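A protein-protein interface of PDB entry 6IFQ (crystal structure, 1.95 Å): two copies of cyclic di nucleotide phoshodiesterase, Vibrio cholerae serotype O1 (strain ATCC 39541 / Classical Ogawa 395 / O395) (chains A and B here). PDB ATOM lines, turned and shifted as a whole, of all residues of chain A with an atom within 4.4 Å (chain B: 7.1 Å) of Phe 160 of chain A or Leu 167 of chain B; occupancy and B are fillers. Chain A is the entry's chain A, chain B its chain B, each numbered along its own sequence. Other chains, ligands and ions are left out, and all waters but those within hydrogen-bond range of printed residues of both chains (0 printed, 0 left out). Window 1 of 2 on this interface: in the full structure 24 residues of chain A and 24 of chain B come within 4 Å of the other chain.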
ATOM      1  N   ASP A 158     -11.557 -17.646  10.132  1.00  0.00           N
ATOM      2  CA  ASP A 158     -12.302 -17.044  11.207  1.00  0.00           C
ATOM      3  C   ASP A 158     -11.480 -15.981  11.955  1.00  0.00           C
ATOM      4  O   ASP A 158     -10.253 -16.045  12.000  1.00  0.00           O
ATOM      5  CB  ASP A 158     -12.751 -18.129  12.167  1.00  0.00           C
ATOM      6  CG  ASP A 158     -13.902 -17.697  13.016  1.00  0.00           C
ATOM      7  OD1 ASP A 158     -14.516 -16.659  12.690  1.00  0.00           O
ATOM      8  OD2 ASP A 158     -14.196 -18.404  14.001  1.00  0.00           O
ATOM      9  N   ASP A 159     -12.179 -15.016  12.539  1.00  0.00           N
ATOM     10  CA  ASP A 159     -11.557 -14.010  13.393  1.00  0.00           C
ATOM     11  C   ASP A 159     -10.450 -13.239  12.685  1.00  0.00           C
ATOM     12  O   ASP A 159      -9.457 -12.858  13.313  1.00  0.00           O
ATOM     13  CB  ASP A 159     -10.997 -14.659  14.662  1.00  0.00           C
ATOM     14  CG  ASP A 159     -12.082 -15.203  15.567  1.00  0.00           C
ATOM     15  OD1 ASP A 159     -13.260 -14.830  15.369  1.00  0.00           O
ATOM     16  OD2 ASP A 159     -11.755 -15.990  16.481  1.00  0.00           O
ATOM     17  N   PHE A 160     -10.629 -13.009  11.387  1.00  0.00           N
ATOM     18  CA  PHE A 160      -9.658 -12.261  10.609  1.00  0.00           C
ATOM     19  C   PHE A 160      -9.404 -10.892  11.225  1.00  0.00           C
ATOM     20  O   PHE A 160     -10.328 -10.079  11.343  1.00  0.00           O
ATOM     21  CB  PHE A 160     -10.126 -12.064   9.178  1.00  0.00           C
ATOM     22  CG  PHE A 160      -9.090 -11.428   8.290  1.00  0.00           C
ATOM     23  CD1 PHE A 160      -8.057 -12.181   7.762  1.00  0.00           C
ATOM     24  CD2 PHE A 160      -9.155 -10.083   7.979  1.00  0.00           C
ATOM     25  CE1 PHE A 160      -7.101 -11.604   6.947  1.00  0.00           C
ATOM     26  CE2 PHE A 160      -8.208  -9.498   7.161  1.00  0.00           C
ATOM     27  CZ  PHE A 160      -7.183 -10.265   6.640  1.00  0.00           C
ATOM     28  N   GLY A 161      -8.156 -10.650  11.608  1.00  0.00           N
ATOM     29  CA  GLY A 161      -7.769  -9.366  12.150  1.00  0.00           C
ATOM     30  C   GLY A 161      -7.543  -9.404  13.645  1.00  0.00           C
ATOM     31  O   GLY A 161      -7.383  -8.353  14.265  1.00  0.00           O
ATOM     32  N   SER A 162      -7.513 -10.597  14.232  1.00  0.00           N
ATOM     33  CA  SER A 162      -7.356 -10.712  15.681  1.00  0.00           C
ATOM     34  C   SER A 162      -6.171 -11.573  16.102  1.00  0.00           C
ATOM     35  O   SER A 162      -5.214 -11.084  16.695  1.00  0.00           O
ATOM     36  CB  SER A 162      -8.620 -11.294  16.301  1.00  0.00           C
ATOM     37  OG  SER A 162      -8.524 -12.705  16.334  1.00  0.00           O
ATOM     38  N   SER A 165      -4.813 -15.521  12.813  1.00  0.00           N
ATOM     39  CA  SER A 165      -5.690 -15.343  11.662  1.00  0.00           C
ATOM     40  C   SER A 165      -5.483 -13.955  11.060  1.00  0.00           C
ATOM     41  O   SER A 165      -6.099 -12.971  11.488  1.00  0.00           O
ATOM     42  CB  SER A 165      -7.152 -15.545  12.069  1.00  0.00           C
ATOM     43  OG  SER A 165      -8.031 -15.039  11.081  1.00  0.00           O
ATOM     44  N   GLY A 166      -4.601 -13.893  10.066  1.00  0.00           N
ATOM     45  CA  GLY A 166      -4.184 -12.637   9.472  1.00  0.00           C
ATOM     46  C   GLY A 166      -3.711 -12.764   8.035  1.00  0.00           C
ATOM     47  O   GLY A 166      -4.037 -13.720   7.332  1.00  0.00           O
ATOM     48  N   LEU A 167      -2.915 -11.792   7.610  1.00  0.00           N
ATOM     49  CA  LEU A 167      -2.562 -11.618   6.209  1.00  0.00           C
ATOM     50  C   LEU A 167      -1.597 -12.672   5.693  1.00  0.00           C
ATOM     51  O   LEU A 167      -1.651 -13.017   4.512  1.00  0.00           O
ATOM     52  CB  LEU A 167      -1.973 -10.214   6.002  1.00  0.00           C
ATOM     53  CG  LEU A 167      -3.023  -9.122   6.226  1.00  0.00           C
ATOM     54  CD1 LEU A 167      -2.414  -7.701   6.385  1.00  0.00           C
ATOM     55  CD2 LEU A 167      -4.079  -9.142   5.133  1.00  0.00           C
ATOM     56  N   LEU A 170      -3.791 -15.511   4.276  1.00  0.00           N
ATOM     57  CA  LEU A 170      -4.338 -15.079   2.992  1.00  0.00           C
ATOM     58  C   LEU A 170      -3.323 -15.110   1.852  1.00  0.00           C
ATOM     59  O   LEU A 170      -3.698 -15.364   0.702  1.00  0.00           O
ATOM     60  CB  LEU A 170      -4.924 -13.674   3.114  1.00  0.00           C
ATOM     61  CG  LEU A 170      -6.417 -13.665   3.422  1.00  0.00           C
ATOM     62  CD1 LEU A 170      -7.014 -12.284   3.158  1.00  0.00           C
ATOM     63  CD2 LEU A 170      -7.085 -14.733   2.585  1.00  0.00           C
ATOM     64  N   VAL A 178     -14.127 -15.062   4.340  1.00  0.00           N
ATOM     65  CA  VAL A 178     -13.332 -14.598   5.468  1.00  0.00           C
ATOM     66  C   VAL A 178     -14.244 -13.881   6.443  1.00  0.00           C
ATOM     67  O   VAL A 178     -14.904 -12.908   6.090  1.00  0.00           O
ATOM     68  CB  VAL A 178     -12.167 -13.662   5.018  1.00  0.00           C
ATOM     69  CG1 VAL A 178     -11.556 -12.969   6.209  1.00  0.00           C
ATOM     70  CG2 VAL A 178     -11.121 -14.483   4.337  1.00  0.00           C
ATOM     71  N   LYS A 179     -14.311 -14.411   7.656  1.00  0.00           N
ATOM     72  CA  LYS A 179     -15.071 -13.793   8.711  1.00  0.00           C
ATOM     73  C   LYS A 179     -14.182 -12.772   9.397  1.00  0.00           C
ATOM     74  O   LYS A 179     -13.170 -13.112   9.997  1.00  0.00           O
ATOM     75  CB  LYS A 179     -15.590 -14.836   9.712  1.00  0.00           C
ATOM     76  CG  LYS A 179     -16.344 -16.018   9.048  1.00  0.00           C
ATOM     77  CD  LYS A 179     -16.868 -17.031  10.089  1.00  0.00           C
ATOM     78  CE  LYS A 179     -18.244 -16.621  10.638  1.00  0.00           C
ATOM     79  NZ  LYS A 179     -18.738 -17.422  11.827  1.00  0.00           N
ATOM     80  N   VAL A 180     -14.587 -11.518   9.299  1.00  0.00           N
ATOM     81  CA  VAL A 180     -13.852 -10.425   9.911  1.00  0.00           C
ATOM     82  C   VAL A 180     -14.220 -10.300  11.387  1.00  0.00           C
ATOM     83  O   VAL A 180     -15.405 -10.247  11.756  1.00  0.00           O
ATOM     84  CB  VAL A 180     -14.124  -9.117   9.173  1.00  0.00           C
ATOM     85  CG1 VAL A 180     -13.498  -7.939   9.931  1.00  0.00           C
ATOM     86  CG2 VAL A 180     -13.579  -9.211   7.750  1.00  0.00           C
ATOM     87  N   ASP A 181     -13.187 -10.292  12.222  1.00  0.00           N
ATOM     88  CA  ASP A 181     -13.320 -10.203  13.671  1.00  0.00           C
ATOM     89  C   ASP A 181     -14.179  -9.018  14.128  1.00  0.00           C
ATOM     90  O   ASP A 181     -14.122  -7.931  13.556  1.00  0.00           O
ATOM     91  CB  ASP A 181     -11.923 -10.115  14.294  1.00  0.00           C
ATOM     92  CG  ASP A 181     -11.958 -10.144  15.795  1.00  0.00           C
ATOM     93  OD1 ASP A 181     -12.104 -11.251  16.361  1.00  0.00           O
ATOM     94  OD2 ASP A 181     -11.844  -9.061  16.404  1.00  0.00           O
ATOM     95  N   LEU A 184     -12.813  -5.310  14.655  1.00  0.00           N
ATOM     96  CA  LEU A 184     -12.762  -4.413  13.503  1.00  0.00           C
ATOM     97  C   LEU A 184     -14.125  -3.837  13.134  1.00  0.00           C
ATOM     98  O   LEU A 184     -14.222  -2.868  12.371  1.00  0.00           O
ATOM     99  CB  LEU A 184     -12.194  -5.155  12.299  1.00  0.00           C
ATOM    100  CG  LEU A 184     -10.751  -5.610  12.445  1.00  0.00           C
ATOM    101  CD1 LEU A 184     -10.272  -6.159  11.128  1.00  0.00           C
ATOM    102  CD2 LEU A 184      -9.883  -4.435  12.918  1.00  0.00           C
ATOM    103  N   ILE A 197      -9.679   0.671   7.300  1.00  0.00           N
ATOM    104  CA  ILE A 197      -9.263  -0.732   7.387  1.00  0.00           C
ATOM    105  C   ILE A 197     -10.213  -1.640   6.616  1.00  0.00           C
ATOM    106  O   ILE A 197      -9.783  -2.462   5.819  1.00  0.00           O
ATOM    107  CB  ILE A 197      -9.165  -1.184   8.865  1.00  0.00           C
ATOM    108  CG1 ILE A 197      -8.004  -0.416   9.545  1.00  0.00           C
ATOM    109  CG2 ILE A 197      -8.983  -2.683   8.988  1.00  0.00           C
ATOM    110  CD1 ILE A 197      -7.712  -0.848  10.960  1.00  0.00           C
ATOM    111  N   CYS A 201      -9.610  -3.584   3.221  1.00  0.00           N
ATOM    112  CA  CYS A 201      -9.721  -5.048   3.272  1.00  0.00           C
ATOM    113  C   CYS A 201     -10.815  -5.575   2.338  1.00  0.00           C
ATOM    114  O   CYS A 201     -10.662  -6.662   1.755  1.00  0.00           O
ATOM    115  CB  CYS A 201     -10.012  -5.548   4.690  1.00  0.00           C
ATOM    116  SG  CYS A 201      -8.584  -5.495   5.840  1.00  0.00           S
ATOM    117  N   PHE A 205     -10.263  -8.464  -0.327  1.00  0.00           N
ATOM    118  CA  PHE A 205     -11.090  -9.673  -0.432  1.00  0.00           C
ATOM    119  C   PHE A 205     -11.658  -9.821  -1.839  1.00  0.00           C
ATOM    120  O   PHE A 205     -11.670 -10.916  -2.411  1.00  0.00           O
ATOM    121  CB  PHE A 205     -12.224  -9.645   0.594  1.00  0.00           C
ATOM    122  CG  PHE A 205     -11.753  -9.614   2.026  1.00  0.00           C
ATOM    123  CD1 PHE A 205     -10.606 -10.288   2.414  1.00  0.00           C
ATOM    124  CD2 PHE A 205     -12.457  -8.907   2.980  1.00  0.00           C
ATOM    125  CE1 PHE A 205     -10.159 -10.242   3.741  1.00  0.00           C
ATOM    126  CE2 PHE A 205     -12.019  -8.860   4.303  1.00  0.00           C
ATOM    127  CZ  PHE A 205     -10.881  -9.537   4.681  1.00  0.00           C
ATOM    128  N   PHE B 160       4.635  -6.901  10.536  1.00  0.00           N
ATOM    129  CA  PHE B 160       3.228  -6.771  10.189  1.00  0.00           C
ATOM    130  C   PHE B 160       2.857  -7.875   9.209  1.00  0.00           C
ATOM    131  O   PHE B 160       3.492  -8.037   8.162  1.00  0.00           O
ATOM    132  CB  PHE B 160       2.917  -5.422   9.572  1.00  0.00           C
ATOM    133  CG  PHE B 160       1.460  -5.220   9.245  1.00  0.00           C
ATOM    134  CD1 PHE B 160       0.538  -4.926  10.246  1.00  0.00           C
ATOM    135  CD2 PHE B 160       1.015  -5.292   7.938  1.00  0.00           C
ATOM    136  CE1 PHE B 160      -0.814  -4.739   9.947  1.00  0.00           C
ATOM    137  CE2 PHE B 160      -0.334  -5.110   7.621  1.00  0.00           C
ATOM    138  CZ  PHE B 160      -1.248  -4.821   8.630  1.00  0.00           C
ATOM    139  N   GLY B 161       1.843  -8.639   9.563  1.00  0.00           N
ATOM    140  CA  GLY B 161       1.358  -9.675   8.675  1.00  0.00           C
ATOM    141  C   GLY B 161       1.640 -11.056   9.215  1.00  0.00           C
ATOM    142  O   GLY B 161       1.124 -12.035   8.694  1.00  0.00           O
ATOM    143  N   TYR B 164       0.646 -12.006  16.099  1.00  0.00           N
ATOM    144  CA  TYR B 164      -0.458 -11.158  16.525  1.00  0.00           C
ATOM    145  C   TYR B 164      -0.192  -9.717  16.113  1.00  0.00           C
ATOM    146  O   TYR B 164      -0.827  -8.788  16.609  1.00  0.00           O
ATOM    147  CB  TYR B 164      -0.671 -11.270  18.034  1.00  0.00           C
ATOM    148  CG  TYR B 164      -1.143 -12.643  18.453  1.00  0.00           C
ATOM    149  CD1 TYR B 164      -2.477 -13.006  18.326  1.00  0.00           C
ATOM    150  CD2 TYR B 164      -0.254 -13.585  18.953  1.00  0.00           C
ATOM    151  CE1 TYR B 164      -2.916 -14.267  18.695  1.00  0.00           C
ATOM    152  CE2 TYR B 164      -0.687 -14.848  19.330  1.00  0.00           C
ATOM    153  CZ  TYR B 164      -2.018 -15.183  19.197  1.00  0.00           C
ATOM    154  OH  TYR B 164      -2.460 -16.436  19.565  1.00  0.00           O
ATOM    155  N   SER B 165       0.749  -9.554  15.188  1.00  0.00           N
ATOM    156  CA  SER B 165       1.063  -8.256  14.609  1.00  0.00           C
ATOM    157  C   SER B 165       0.263  -8.013  13.336  1.00  0.00           C
ATOM    158  O   SER B 165       0.781  -8.154  12.229  1.00  0.00           O
ATOM    159  CB  SER B 165       2.558  -8.154  14.317  1.00  0.00           C
ATOM    160  OG  SER B 165       2.815  -7.086  13.428  1.00  0.00           O
ATOM    161  N   GLY B 166      -1.006  -7.648  13.501  1.00  0.00           N
ATOM    162  CA  GLY B 166      -1.884  -7.438  12.367  1.00  0.00           C
ATOM    163  C   GLY B 166      -2.797  -6.235  12.482  1.00  0.00           C
ATOM    164  O   GLY B 166      -2.475  -5.239  13.120  1.00  0.00           O
ATOM    165  N   LEU B 167      -3.964  -6.348  11.863  1.00  0.00           N
ATOM    166  CA  LEU B 167      -4.879  -5.230  11.711  1.00  0.00           C
ATOM    167  C   LEU B 167      -5.502  -4.734  13.008  1.00  0.00           C
ATOM    168  O   LEU B 167      -5.952  -3.588  13.075  1.00  0.00           O
ATOM    169  CB  LEU B 167      -5.986  -5.625  10.731  1.00  0.00           C
ATOM    170  CG  LEU B 167      -5.358  -5.940   9.378  1.00  0.00           C
ATOM    171  CD1 LEU B 167      -6.283  -6.812   8.523  1.00  0.00           C
ATOM    172  CD2 LEU B 167      -4.986  -4.672   8.650  1.00  0.00           C
ATOM    173  N   ASN B 168      -5.553  -5.590  14.024  1.00  0.00           N
ATOM    174  CA  ASN B 168      -6.116  -5.197  15.311  1.00  0.00           C
ATOM    175  C   ASN B 168      -5.286  -4.087  15.962  1.00  0.00           C
ATOM    176  O   ASN B 168      -5.820  -3.210  16.638  1.00  0.00           O
ATOM    177  CB  ASN B 168      -6.206  -6.399  16.245  1.00  0.00           C
ATOM    178  CG  ASN B 168      -4.874  -7.113  16.409  1.00  0.00           C
ATOM    179  OD1 ASN B 168      -4.041  -7.130  15.499  1.00  0.00           O
ATOM    180  ND2 ASN B 168      -4.670  -7.714  17.575  1.00  0.00           N
ATOM    181  N   LEU B 169      -3.977  -4.125  15.736  1.00  0.00           N
ATOM    182  CA  LEU B 169      -3.097  -3.100  16.250  1.00  0.00           C
ATOM    183  C   LEU B 169      -3.448  -1.772  15.594  1.00  0.00           C
ATOM    184  O   LEU B 169      -3.815  -0.807  16.285  1.00  0.00           O
ATOM    185  CB  LEU B 169      -1.630  -3.465  16.005  1.00  0.00           C
ATOM    186  CG  LEU B 169      -1.179  -4.735  16.732  1.00  0.00           C
ATOM    187  CD1 LEU B 169       0.327  -4.941  16.623  1.00  0.00           C
ATOM    188  CD2 LEU B 169      -1.624  -4.707  18.187  1.00  0.00           C
ATOM    189  N   LEU B 170      -3.386  -1.747  14.263  1.00  0.00           N
ATOM    190  CA  LEU B 170      -3.637  -0.524  13.506  1.00  0.00           C
ATOM    191  C   LEU B 170      -4.962   0.113  13.891  1.00  0.00           C
ATOM    192  O   LEU B 170      -5.102   1.330  13.846  1.00  0.00           O
ATOM    193  CB  LEU B 170      -3.629  -0.790  11.999  1.00  0.00           C
ATOM    194  CG  LEU B 170      -2.308  -1.221  11.350  1.00  0.00           C
ATOM    195  CD1 LEU B 170      -2.157  -0.623   9.967  1.00  0.00           C
ATOM    196  CD2 LEU B 170      -1.139  -0.820  12.188  1.00  0.00           C
ATOM    197  N   ALA B 171      -5.927  -0.720  14.278  1.00  0.00           N
ATOM    198  CA  ALA B 171      -7.272  -0.255  14.559  1.00  0.00           C
ATOM    199  C   ALA B 171      -7.382   0.758  15.709  1.00  0.00           C
ATOM    200  O   ALA B 171      -8.228   1.646  15.656  1.00  0.00           O
ATOM    201  CB  ALA B 171      -8.178  -1.451  14.847  1.00  0.00           C
ATOM    202  N   ASP B 172      -6.561   0.617  16.746  1.00  0.00           N
ATOM    203  CA  ASP B 172      -6.708   1.457  17.935  1.00  0.00           C
ATOM    204  C   ASP B 172      -5.597   2.480  18.115  1.00  0.00           C
ATOM    205  O   ASP B 172      -5.736   3.422  18.897  1.00  0.00           O
ATOM    206  CB  ASP B 172      -6.808   0.577  19.174  1.00  0.00           C
ATOM    207  CG  ASP B 172      -8.157  -0.132  19.271  1.00  0.00           C
ATOM    208  OD1 ASP B 172      -9.192   0.530  19.028  1.00  0.00           O
ATOM    209  OD2 ASP B 172      -8.185  -1.342  19.582  1.00  0.00           O
ATOM    210  N   PHE B 173      -4.491   2.289  17.403  1.00  0.00           N
ATOM    211  CA  PHE B 173      -3.424   3.290  17.381  1.00  0.00           C
ATOM    212  C   PHE B 173      -2.561   3.111  16.136  1.00  0.00           C
ATOM    213  O   PHE B 173      -2.619   2.073  15.458  1.00  0.00           O
ATOM    214  CB  PHE B 173      -2.559   3.211  18.645  1.00  0.00           C
ATOM    215  CG  PHE B 173      -1.766   1.941  18.748  1.00  0.00           C
ATOM    216  CD1 PHE B 173      -2.330   0.796  19.300  1.00  0.00           C
ATOM    217  CD2 PHE B 173      -0.467   1.881  18.271  1.00  0.00           C
ATOM    218  CE1 PHE B 173      -1.600  -0.374  19.387  1.00  0.00           C
ATOM    219  CE2 PHE B 173       0.265   0.709  18.349  1.00  0.00           C
ATOM    220  CZ  PHE B 173      -0.295  -0.417  18.907  1.00  0.00           C
ATOM    221  N   CYS B 201      -2.790  -2.870   1.319  1.00  0.00           N
ATOM    222  CA  CYS B 201      -2.203  -2.481   2.586  1.00  0.00           C
ATOM    223  C   CYS B 201      -1.489  -1.129   2.466  1.00  0.00           C
ATOM    224  O   CYS B 201      -1.461  -0.356   3.422  1.00  0.00           O
ATOM    225  CB  CYS B 201      -1.209  -3.525   3.080  1.00  0.00           C
ATOM    226  SG  CYS B 201      -1.948  -4.985   3.879  1.00  0.00           S
ATOM    227  N   LEU B 204      -4.029   1.442   2.671  1.00  0.00           N
ATOM    228  CA  LEU B 204      -4.468   1.550   4.054  1.00  0.00           C
ATOM    229  C   LEU B 204      -3.459   2.399   4.865  1.00  0.00           C
ATOM    230  O   LEU B 204      -3.851   3.275   5.630  1.00  0.00           O
ATOM    231  CB  LEU B 204      -4.629   0.163   4.670  1.00  0.00           C
ATOM    232  CG  LEU B 204      -5.214   0.001   6.073  1.00  0.00           C
ATOM    233  CD1 LEU B 204      -4.142  -0.162   7.101  1.00  0.00           C
ATOM    234  CD2 LEU B 204      -6.132   1.165   6.451  1.00  0.00           C
ATOM    235  N   PHE B 205      -2.185   2.085   4.696  1.00  0.00           N
ATOM    236  CA  PHE B 205      -1.088   2.785   5.384  1.00  0.00           C
ATOM    237  C   PHE B 205      -1.143   4.266   5.087  1.00  0.00           C
ATOM    238  O   PHE B 205      -0.974   5.084   5.988  1.00  0.00           O
ATOM    239  CB  PHE B 205       0.273   2.227   4.967  1.00  0.00           C
ATOM    240  CG  PHE B 205       0.503   0.800   5.385  1.00  0.00           C
ATOM    241  CD1 PHE B 205      -0.143   0.277   6.499  1.00  0.00           C
ATOM    242  CD2 PHE B 205       1.359  -0.021   4.673  1.00  0.00           C
ATOM    243  CE1 PHE B 205       0.048  -1.050   6.883  1.00  0.00           C
ATOM    244  CE2 PHE B 205       1.572  -1.329   5.066  1.00  0.00           C
ATOM    245  CZ  PHE B 205       0.905  -1.852   6.177  1.00  0.00           C
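Of the 17 printed residues of chain A, 7 touch a printed residue of chain B.
Printed residues of chain B that touch a printed residue of chain A: Phe 160, Tyr 164, Leu 167, Asn 168, Ala 171, Cys 201 and Leu 204.
Hydrophobic or aromatic side chains of chain B that line the printed part of chain A: Phe 160, Tyr 164, Leu 167, Ala 171 and Leu 204.
The backbone NH (N) of Phe 160 of chain B sits close to the side-chain hydroxyl (OG) of Ser 165 of chain B (3.4 Å).
OD1 of Asn 168 of chain B sits close to O of Gly 166 of chain B, at 3.4 Å.
The side-chain hydroxyl (OG) of Ser 162 of chain A is in hydrogen-bond range of the backbone carbonyl oxygen (O) of Asp 159 of chain A (3.2 Å).
The side-chain hydroxyl (OG) of Ser 165 of chain A lies close to the backbone NH (N) of Phe 160 of chain A (3.3 Å).
The backbone NH (N) of Phe 160 of chain A sits at hydrogen-bond distance from the backbone carbonyl oxygen (O) of Lys 179 of chain A, 2.9 Å away.
The backbone NH (N) of Asp 181 of chain A is in hydrogen-bond range of the backbone carbonyl oxygen (O) of Phe 160 of chain A (3.0 Å).
N of Asn 168 of chain B sits close to O of Gly 161 of chain A (3.3 Å).
Among the printed residues, merely in contact across the chains: Ser 162 of chain A with Asn 168 of chain B (3.5 Å), Leu 167 of chain A with Phe 160 of chain B (3.5 Å), Phe 160 of chain A with Leu 167 of chain B (3.6 Å), Ile 197 of chain A with Ala 171 of chain B (3.7 Å), Ile 197 of chain A with Leu 204 of chain B (3.7 Å), Ser 162 of chain A with Tyr 164 of chain B (3.7 Å), Leu 167 of chain A with Cys 201 of chain B (3.7 Å), Cys 201 of chain A with Leu 167 of chain B (3.8 Å), Ile 197 of chain A with Leu 167 of chain B (3.9 Å) and Leu 184 of chain A with Ala 171 of chain B (3.9 Å).
Phe 160 of chain A touches Leu 167 of chain B, and with the chains exchanged Leu 167 of chain A touches Phe 160 of chain B.
Leu 167 of chain A touches Cys 201 of chain B, and with the chains exchanged Cys 201 of chain A touches Leu 167 of chain B.
Positions printed for both chains: 160, 161, 165, 166, 167, 170, 201 and 205.
Of the 11 pairs that touch across the chains among the printed residues, 4 have their exchanged pair printed and touching as well.
Of chain B, only Leu 167 (3.6 Å) comes within 4 Å of Phe 160 of chain A.
Of the printed residues of chain B, Ser 162 of chain A touches Tyr 164 (3.7 Å) and Asn 168 (3.5 Å).
Of the printed residues of chain B, Leu 184 of chain A touches Ala 171.
Printed residues of chain B within 4 Å of Ile 197 of chain A: Leu 167 (3.9 Å), Ala 171 (3.7 Å) and Leu 204 (3.7 Å).
Of the printed residues of chain B, Cys 201 of chain A touches Leu 167.
Of the printed residues of chain A, Leu 167 of chain B touches Phe 160 (3.6 Å), Ile 197 (3.9 Å) and Cys 201 (3.8 Å).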
